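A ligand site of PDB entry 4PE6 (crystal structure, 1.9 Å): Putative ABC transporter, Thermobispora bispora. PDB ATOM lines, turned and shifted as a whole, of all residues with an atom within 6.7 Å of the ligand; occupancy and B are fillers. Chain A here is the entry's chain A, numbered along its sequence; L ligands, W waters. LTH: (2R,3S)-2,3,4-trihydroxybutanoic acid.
The side-chain carboxylate (OD2) of Asp 113 lies within hydrogen-bond range of the side-chain amide nitrogen (ND2) of Asn 88, 2.9 Å away.
The side-chain amide nitrogen of Gln 263 sits at hydrogen-bond distance from the side-chain carboxylate of Asp 113, at 3.0 Å.
O of Ser 259 sits at hydrogen-bond distance from NE1 of Trp 32, at 2.9 Å.
The backbone NH (N) of Arg 33 is in hydrogen-bond range of the side-chain amide oxygen (OD1) of Asn 30 (2.8 Å).
The side-chain amide nitrogen (ND2) of Asn 30 is in hydrogen-bond range of the backbone carbonyl oxygen (O) of Met 187 (3.1 Å).
OD1 of Asn 88 is in hydrogen-bond range of NH1 of Arg 33, 3.3 Å away.
The side-chain sulfur of Cys 213 is disulfide-bonded to the side-chain sulfur of Cys 188 (2.0 Å).
OG of Ser 158 sits at hydrogen-bond distance from O of Val 155 (2.6 Å).
Water W2 lies within hydrogen-bond range of an oxygen (O3) of the ligand (2.7 Å), the backbone NH (N) of Val 155 (2.8 Å) and the side-chain sulfur (SG) of Cys 188 (3.6 Å).
Water W1 lies within hydrogen-bond range of OG of Ser 158, O3 of the ligand and NH2 of Arg 33.
An oxygen (O1) of the ligand lies close to the side-chain sulfur of Cys 188 (3.6 Å).
CE3 of Trp 32 touches C1 of the ligand, at 3.5 Å.
Phe 128 touches the ligand (CE1 to O4, 3.6 Å).
Trp 131 touches the ligand (CZ3 to O4, 3.5 Å).
CG2 of Val 155 touches O of the ligand, 3.6 Å away.
Pro 160 touches the ligand.
Met 258 touches the ligand (CE to O1, 3.6 Å).
Hydrophobic or aromatic side chains that line the ligand: Trp 32, Phe 128, Trp 131, Val 155, Pro 160 and Met 258.
The side-chain carboxylate (OD1) of Asp 113 lies within hydrogen-bond range of an oxygen (O4) of the ligand.
An oxygen (O4) of the ligand sits at hydrogen-bond distance from the side-chain hydroxyl of Ser 259 (2.6 Å).
O of the ligand is in hydrogen-bond range of ND2 of Asn 30 (2.9 Å).
NE of Arg 33 lies within salt-bridge range of O of the ligand.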
ATOM      1  N   PHE A  27      11.857  -6.102 -18.685  1.00  0.00           N
ATOM      2  CA  PHE A  27      12.213  -7.363 -19.334  1.00  0.00           C
ATOM      3  C   PHE A  27      11.045  -8.297 -19.242  1.00  0.00           C
ATOM      4  O   PHE A  27      10.503  -8.495 -18.157  1.00  0.00           O
ATOM      5  CB  PHE A  27      13.446  -8.015 -18.684  1.00  0.00           C
ATOM      6  CG  PHE A  27      13.860  -9.303 -19.356  1.00  0.00           C
ATOM      7  CD1 PHE A  27      14.247  -9.316 -20.693  1.00  0.00           C
ATOM      8  CD2 PHE A  27      13.845 -10.503 -18.662  1.00  0.00           C
ATOM      9  CE1 PHE A  27      14.620 -10.501 -21.313  1.00  0.00           C
ATOM     10  CE2 PHE A  27      14.225 -11.690 -19.289  1.00  0.00           C
ATOM     11  CZ  PHE A  27      14.614 -11.682 -20.614  1.00  0.00           C
ATOM     12  N   ASN A  30      11.051 -13.968 -19.894  1.00  0.00           N
ATOM     13  CA  ASN A  30      11.056 -15.180 -19.092  1.00  0.00           C
ATOM     14  C   ASN A  30       9.686 -15.371 -18.460  1.00  0.00           C
ATOM     15  O   ASN A  30       8.866 -14.442 -18.387  1.00  0.00           O
ATOM     16  CB  ASN A  30      12.227 -15.220 -18.064  1.00  0.00           C
ATOM     17  CG  ASN A  30      11.979 -14.346 -16.827  1.00  0.00           C
ATOM     18  OD1 ASN A  30      10.868 -14.296 -16.302  1.00  0.00           O
ATOM     19  ND2 ASN A  30      13.029 -13.685 -16.337  1.00  0.00           N
ATOM     20  N   TRP A  32       8.728 -16.022 -15.442  1.00  0.00           N
ATOM     21  CA  TRP A  32       8.504 -15.356 -14.152  1.00  0.00           C
ATOM     22  C   TRP A  32       7.885 -13.977 -14.416  1.00  0.00           C
ATOM     23  O   TRP A  32       6.900 -13.579 -13.781  1.00  0.00           O
ATOM     24  CB  TRP A  32       9.827 -15.277 -13.354  1.00  0.00           C
ATOM     25  CG  TRP A  32       9.715 -14.701 -11.962  1.00  0.00           C
ATOM     26  CD1 TRP A  32       9.676 -15.391 -10.801  1.00  0.00           C
ATOM     27  CD2 TRP A  32       9.670 -13.303 -11.603  1.00  0.00           C
ATOM     28  NE1 TRP A  32       9.555 -14.523  -9.736  1.00  0.00           N
ATOM     29  CE2 TRP A  32       9.577 -13.238 -10.199  1.00  0.00           C
ATOM     30  CE3 TRP A  32       9.670 -12.114 -12.324  1.00  0.00           C
ATOM     31  CZ2 TRP A  32       9.494 -12.036  -9.508  1.00  0.00           C
ATOM     32  CZ3 TRP A  32       9.602 -10.923 -11.659  1.00  0.00           C
ATOM     33  CH2 TRP A  32       9.526 -10.883 -10.247  1.00  0.00           C
ATOM     34  N   ARG A  33       8.436 -13.254 -15.389  1.00  0.00           N
ATOM     35  CA  ARG A  33       7.970 -11.915 -15.719  1.00  0.00           C
ATOM     36  C   ARG A  33       6.570 -11.971 -16.329  1.00  0.00           C
ATOM     37  O   ARG A  33       5.775 -11.063 -16.126  1.00  0.00           O
ATOM     38  CB  ARG A  33       8.929 -11.236 -16.677  1.00  0.00           C
ATOM     39  CG  ARG A  33      10.273 -10.855 -16.093  1.00  0.00           C
ATOM     40  CD  ARG A  33      10.207  -9.680 -15.095  1.00  0.00           C
ATOM     41  NE  ARG A  33      11.550  -9.408 -14.603  1.00  0.00           N
ATOM     42  CZ  ARG A  33      12.268  -8.303 -14.821  1.00  0.00           C
ATOM     43  NH1 ARG A  33      11.785  -7.278 -15.460  1.00  0.00           N
ATOM     44  NH2 ARG A  33      13.497  -8.224 -14.359  1.00  0.00           N
ATOM     45  N   MET A  36       4.296 -12.352 -13.477  1.00  0.00           N
ATOM     46  CA  MET A  36       4.241 -11.070 -12.775  1.00  0.00           C
ATOM     47  C   MET A  36       3.261 -10.139 -13.431  1.00  0.00           C
ATOM     48  O   MET A  36       2.482  -9.474 -12.749  1.00  0.00           O
ATOM     49  CB  MET A  36       5.660 -10.494 -12.728  1.00  0.00           C
ATOM     50  CG  MET A  36       5.600  -9.028 -12.370  1.00  0.00           C
ATOM     51  SD  MET A  36       7.365  -8.265 -12.716  1.00  0.00           S
ATOM     52  CE  MET A  36       6.882  -7.669 -14.517  1.00  0.00           C
ATOM     53  N   ASN A  88       9.368  -1.933 -13.015  1.00  0.00           N
ATOM     54  CA  ASN A  88      10.406  -2.946 -12.868  1.00  0.00           C
ATOM     55  C   ASN A  88      11.570  -2.521 -13.769  1.00  0.00           C
ATOM     56  O   ASN A  88      11.532  -2.667 -15.015  1.00  0.00           O
ATOM     57  CB  ASN A  88       9.899  -4.340 -13.192  1.00  0.00           C
ATOM     58  CG  ASN A  88      10.877  -5.443 -12.787  1.00  0.00           C
ATOM     59  OD1 ASN A  88      12.081  -5.268 -12.897  1.00  0.00           O
ATOM     60  ND2 ASN A  88      10.348  -6.582 -12.331  1.00  0.00           N
ATOM     61  N   ASP A 113      10.409  -5.030  -7.425  1.00  0.00           N
ATOM     62  CA  ASP A 113      11.314  -6.121  -7.793  1.00  0.00           C
ATOM     63  C   ASP A 113      12.701  -5.594  -8.123  1.00  0.00           C
ATOM     64  O   ASP A 113      13.368  -6.089  -9.038  1.00  0.00           O
ATOM     65  CB  ASP A 113      10.727  -6.901  -8.981  1.00  0.00           C
ATOM     66  CG  ASP A 113      11.541  -8.139  -9.322  1.00  0.00           C
ATOM     67  OD1 ASP A 113      11.906  -8.872  -8.379  1.00  0.00           O
ATOM     68  OD2 ASP A 113      11.812  -8.381 -10.527  1.00  0.00           O
ATOM     69  N   SER A 114      13.119  -4.581  -7.367  1.00  0.00           N
ATOM     70  CA  SER A 114      14.419  -3.949  -7.491  1.00  0.00           C
ATOM     71  C   SER A 114      14.562  -2.907  -6.386  1.00  0.00           C
ATOM     72  O   SER A 114      13.559  -2.425  -5.845  1.00  0.00           O
ATOM     73  CB  SER A 114      14.583  -3.242  -8.830  1.00  0.00           C
ATOM     74  OG  SER A 114      14.997  -4.160  -9.850  1.00  0.00           O
ATOM     75  N   ASN A 126      12.102  -7.836  -2.888  1.00  0.00           N
ATOM     76  CA  ASN A 126      12.301  -9.032  -2.112  1.00  0.00           C
ATOM     77  C   ASN A 126      13.761  -9.060  -1.696  1.00  0.00           C
ATOM     78  O   ASN A 126      14.598  -8.342  -2.270  1.00  0.00           O
ATOM     79  CB  ASN A 126      12.019 -10.307  -2.935  1.00  0.00           C
ATOM     80  CG  ASN A 126      10.533 -10.651  -3.126  1.00  0.00           C
ATOM     81  OD1 ASN A 126      10.215 -11.679  -3.753  1.00  0.00           O
ATOM     82  ND2 ASN A 126       9.618  -9.803  -2.661  1.00  0.00           N
ATOM     83  N   PHE A 128      16.893 -10.363  -2.416  1.00  0.00           N
ATOM     84  CA  PHE A 128      17.662 -11.061  -3.443  1.00  0.00           C
ATOM     85  C   PHE A 128      18.823 -11.806  -2.831  1.00  0.00           C
ATOM     86  O   PHE A 128      19.174 -12.893  -3.280  1.00  0.00           O
ATOM     87  CB  PHE A 128      18.068 -10.081  -4.529  1.00  0.00           C
ATOM     88  CG  PHE A 128      16.919  -9.288  -5.052  1.00  0.00           C
ATOM     89  CD1 PHE A 128      15.822  -9.953  -5.617  1.00  0.00           C
ATOM     90  CD2 PHE A 128      16.874  -7.926  -4.929  1.00  0.00           C
ATOM     91  CE1 PHE A 128      14.733  -9.239  -6.065  1.00  0.00           C
ATOM     92  CE2 PHE A 128      15.798  -7.215  -5.391  1.00  0.00           C
ATOM     93  CZ  PHE A 128      14.714  -7.868  -5.945  1.00  0.00           C
ATOM     94  N   TRP A 131      17.436 -15.157  -1.551  1.00  0.00           N
ATOM     95  CA  TRP A 131      17.214 -16.031  -2.713  1.00  0.00           C
ATOM     96  C   TRP A 131      18.526 -16.631  -3.150  1.00  0.00           C
ATOM     97  O   TRP A 131      18.688 -17.845  -3.176  1.00  0.00           O
ATOM     98  CB  TRP A 131      16.551 -15.247  -3.835  1.00  0.00           C
ATOM     99  CG  TRP A 131      16.387 -15.959  -5.159  1.00  0.00           C
ATOM    100  CD1 TRP A 131      16.738 -17.241  -5.480  1.00  0.00           C
ATOM    101  CD2 TRP A 131      15.853 -15.390  -6.351  1.00  0.00           C
ATOM    102  NE1 TRP A 131      16.427 -17.509  -6.816  1.00  0.00           N
ATOM    103  CE2 TRP A 131      15.888 -16.385  -7.360  1.00  0.00           C
ATOM    104  CE3 TRP A 131      15.352 -14.123  -6.673  1.00  0.00           C
ATOM    105  CZ2 TRP A 131      15.440 -16.153  -8.666  1.00  0.00           C
ATOM    106  CZ3 TRP A 131      14.894 -13.903  -7.972  1.00  0.00           C
ATOM    107  CH2 TRP A 131      14.928 -14.927  -8.947  1.00  0.00           C
ATOM    108  N   GLY A 154      21.232 -14.628 -14.007  1.00  0.00           N
ATOM    109  CA  GLY A 154      19.837 -14.238 -14.250  1.00  0.00           C
ATOM    110  C   GLY A 154      19.658 -13.103 -15.236  1.00  0.00           C
ATOM    111  O   GLY A 154      20.239 -13.123 -16.336  1.00  0.00           O
ATOM    112  N   VAL A 155      18.832 -12.138 -14.863  1.00  0.00           N
ATOM    113  CA  VAL A 155      18.508 -11.008 -15.722  1.00  0.00           C
ATOM    114  C   VAL A 155      19.663  -9.999 -15.686  1.00  0.00           C
ATOM    115  O   VAL A 155      19.580  -8.956 -15.048  1.00  0.00           O
ATOM    116  CB  VAL A 155      17.151 -10.377 -15.364  1.00  0.00           C
ATOM    117  CG1 VAL A 155      16.755  -9.282 -16.330  1.00  0.00           C
ATOM    118  CG2 VAL A 155      16.060 -11.472 -15.419  1.00  0.00           C
ATOM    119  N   SER A 158      20.181  -6.027 -14.797  1.00  0.00           N
ATOM    120  CA  SER A 158      19.315  -5.577 -13.700  1.00  0.00           C
ATOM    121  C   SER A 158      20.047  -5.501 -12.333  1.00  0.00           C
ATOM    122  O   SER A 158      21.073  -6.143 -12.106  1.00  0.00           O
ATOM    123  CB  SER A 158      18.055  -6.470 -13.580  1.00  0.00           C
ATOM    124  OG  SER A 158      18.378  -7.742 -13.048  1.00  0.00           O
ATOM    125  N   PRO A 160      18.855  -6.544  -9.223  1.00  0.00           N
ATOM    126  CA  PRO A 160      18.845  -7.781  -8.473  1.00  0.00           C
ATOM    127  C   PRO A 160      19.837  -8.811  -8.981  1.00  0.00           C
ATOM    128  O   PRO A 160      20.469  -9.486  -8.183  1.00  0.00           O
ATOM    129  CB  PRO A 160      17.396  -8.292  -8.636  1.00  0.00           C
ATOM    130  CG  PRO A 160      16.602  -7.078  -8.925  1.00  0.00           C
ATOM    131  CD  PRO A 160      17.523  -6.189  -9.722  1.00  0.00           C
ATOM    132  N   GLU A 161      19.976  -8.952 -10.295  1.00  0.00           N
ATOM    133  CA  GLU A 161      20.924  -9.929 -10.829  1.00  0.00           C
ATOM    134  C   GLU A 161      22.341  -9.607 -10.388  1.00  0.00           C
ATOM    135  O   GLU A 161      23.100 -10.503  -9.987  1.00  0.00           O
ATOM    136  CB  GLU A 161      20.875  -9.999 -12.345  1.00  0.00           C
ATOM    137  CG  GLU A 161      21.646 -11.198 -12.895  1.00  0.00           C
ATOM    138  CD  GLU A 161      23.157 -11.025 -12.913  1.00  0.00           C
ATOM    139  OE1 GLU A 161      23.632  -9.876 -13.096  1.00  0.00           O
ATOM    140  OE2 GLU A 161      23.866 -12.069 -12.773  1.00  0.00           O
ATOM    141  N   MET A 164      22.730 -10.624  -6.739  1.00  0.00           N
ATOM    142  CA  MET A 164      22.743 -12.060  -6.538  1.00  0.00           C
ATOM    143  C   MET A 164      24.007 -12.671  -7.021  1.00  0.00           C
ATOM    144  O   MET A 164      24.501 -13.598  -6.392  1.00  0.00           O
ATOM    145  CB  MET A 164      21.504 -12.716  -7.173  1.00  0.00           C
ATOM    146  CG  MET A 164      20.254 -12.152  -6.496  1.00  0.00           C
ATOM    147  SD  MET A 164      18.605 -13.198  -6.858  1.00  0.00           S
ATOM    148  CE  MET A 164      18.086 -12.471  -8.567  1.00  0.00           C
ATOM    149  N   MET A 187      19.155 -15.465 -18.201  1.00  0.00           N
ATOM    150  CA  MET A 187      18.004 -14.529 -18.116  1.00  0.00           C
ATOM    151  C   MET A 187      16.817 -15.079 -17.299  1.00  0.00           C
ATOM    152  O   MET A 187      15.689 -14.661 -17.495  1.00  0.00           O
ATOM    153  CB  MET A 187      17.533 -14.060 -19.509  1.00  0.00           C
ATOM    154  CG  MET A 187      18.641 -13.544 -20.427  1.00  0.00           C
ATOM    155  SD  MET A 187      19.532 -11.916 -19.729  1.00  0.00           S
ATOM    156  CE  MET A 187      18.093 -10.613 -19.964  1.00  0.00           C
ATOM    157  N   CYS A 188      17.088 -15.987 -16.353  1.00  0.00           N
ATOM    158  CA  CYS A 188      16.053 -16.758 -15.609  1.00  0.00           C
ATOM    159  C   CYS A 188      15.011 -17.368 -16.543  1.00  0.00           C
ATOM    160  O   CYS A 188      13.827 -17.461 -16.217  1.00  0.00           O
ATOM    161  CB  CYS A 188      15.365 -15.941 -14.526  1.00  0.00           C
ATOM    162  SG  CYS A 188      16.458 -14.864 -13.582  1.00  0.00           S
ATOM    163  N   CYS A 213      19.144 -19.256 -11.915  1.00  0.00           N
ATOM    164  CA  CYS A 213      18.057 -18.357 -11.573  1.00  0.00           C
ATOM    165  C   CYS A 213      16.758 -18.964 -12.108  1.00  0.00           C
ATOM    166  O   CYS A 213      16.386 -18.712 -13.256  1.00  0.00           O
ATOM    167  CB  CYS A 213      18.284 -17.000 -12.218  1.00  0.00           C
ATOM    168  SG  CYS A 213      16.992 -15.789 -11.860  1.00  0.00           S
ATOM    169  N   MET A 258      12.501 -18.662  -5.684  1.00  0.00           N
ATOM    170  CA  MET A 258      12.557 -17.463  -6.507  1.00  0.00           C
ATOM    171  C   MET A 258      11.907 -16.348  -5.734  1.00  0.00           C
ATOM    172  O   MET A 258      11.238 -16.577  -4.712  1.00  0.00           O
ATOM    173  CB  MET A 258      11.785 -17.587  -7.845  1.00  0.00           C
ATOM    174  CG  MET A 258      12.323 -18.684  -8.734  1.00  0.00           C
ATOM    175  SD  MET A 258      11.643 -18.559 -10.575  1.00  0.00           S
ATOM    176  CE  MET A 258      12.848 -17.117 -11.221  1.00  0.00           C
ATOM    177  N   SER A 259      12.133 -15.130  -6.180  1.00  0.00           N
ATOM    178  CA  SER A 259      11.332 -13.981  -5.792  1.00  0.00           C
ATOM    179  C   SER A 259       9.859 -14.183  -6.144  1.00  0.00           C
ATOM    180  O   SER A 259       9.504 -15.101  -6.930  1.00  0.00           O
ATOM    181  CB  SER A 259      11.863 -12.719  -6.472  1.00  0.00           C
ATOM    182  OG  SER A 259      11.825 -12.872  -7.887  1.00  0.00           O
ATOM    183  N   ASP A 260       9.033 -13.283  -5.615  1.00  0.00           N
ATOM    184  CA  ASP A 260       7.581 -13.301  -5.770  1.00  0.00           C
ATOM    185  C   ASP A 260       7.150 -12.473  -6.957  1.00  0.00           C
ATOM    186  O   ASP A 260       7.322 -11.251  -6.943  1.00  0.00           O
ATOM    187  CB  ASP A 260       6.952 -12.736  -4.490  1.00  0.00           C
ATOM    188  CG  ASP A 260       5.433 -12.639  -4.536  1.00  0.00           C
ATOM    189  OD1 ASP A 260       4.753 -13.379  -5.298  1.00  0.00           O
ATOM    190  OD2 ASP A 260       4.901 -11.818  -3.770  1.00  0.00           O
ATOM    191  N   GLN A 263       4.982  -9.286  -6.460  1.00  0.00           N
ATOM    192  CA  GLN A 263       5.413  -7.948  -6.114  1.00  0.00           C
ATOM    193  C   GLN A 263       4.676  -6.889  -6.927  1.00  0.00           C
ATOM    194  O   GLN A 263       4.469  -5.783  -6.425  1.00  0.00           O
ATOM    195  CB  GLN A 263       6.894  -7.768  -6.320  1.00  0.00           C
ATOM    196  CG  GLN A 263       7.756  -8.429  -5.254  1.00  0.00           C
ATOM    197  CD  GLN A 263       9.211  -8.373  -5.660  1.00  0.00           C
ATOM    198  OE1 GLN A 263       9.911  -7.448  -5.274  1.00  0.00           O
ATOM    199  NE2 GLN A 263       9.663  -9.357  -6.472  1.00  0.00           N
HETATM  200  O1  LTH L   1      13.233 -13.758 -12.557  1.00  0.00           O
HETATM  201  C1  LTH L   1      13.080 -12.509 -12.801  1.00  0.00           C
HETATM  202  O   LTH L   1      12.862 -12.002 -13.923  1.00  0.00           O
HETATM  203  C2  LTH L   1      13.088 -11.517 -11.606  1.00  0.00           C
HETATM  204  O2  LTH L   1      12.960 -10.142 -12.065  1.00  0.00           O
HETATM  205  C3  LTH L   1      14.366 -11.615 -10.801  1.00  0.00           C
HETATM  206  O3  LTH L   1      15.491 -11.342 -11.637  1.00  0.00           O
HETATM  207  C4  LTH L   1      14.328 -10.563  -9.679  1.00  0.00           C
HETATM  208  O4  LTH L   1      13.232 -10.951  -8.805  1.00  0.00           O
HETATM  209  O   HOH W   1      15.909  -8.615 -12.267  1.00  0.00           O
HETATM  210  O   HOH W   2      18.075 -12.007 -12.151  1.00  0.00           O
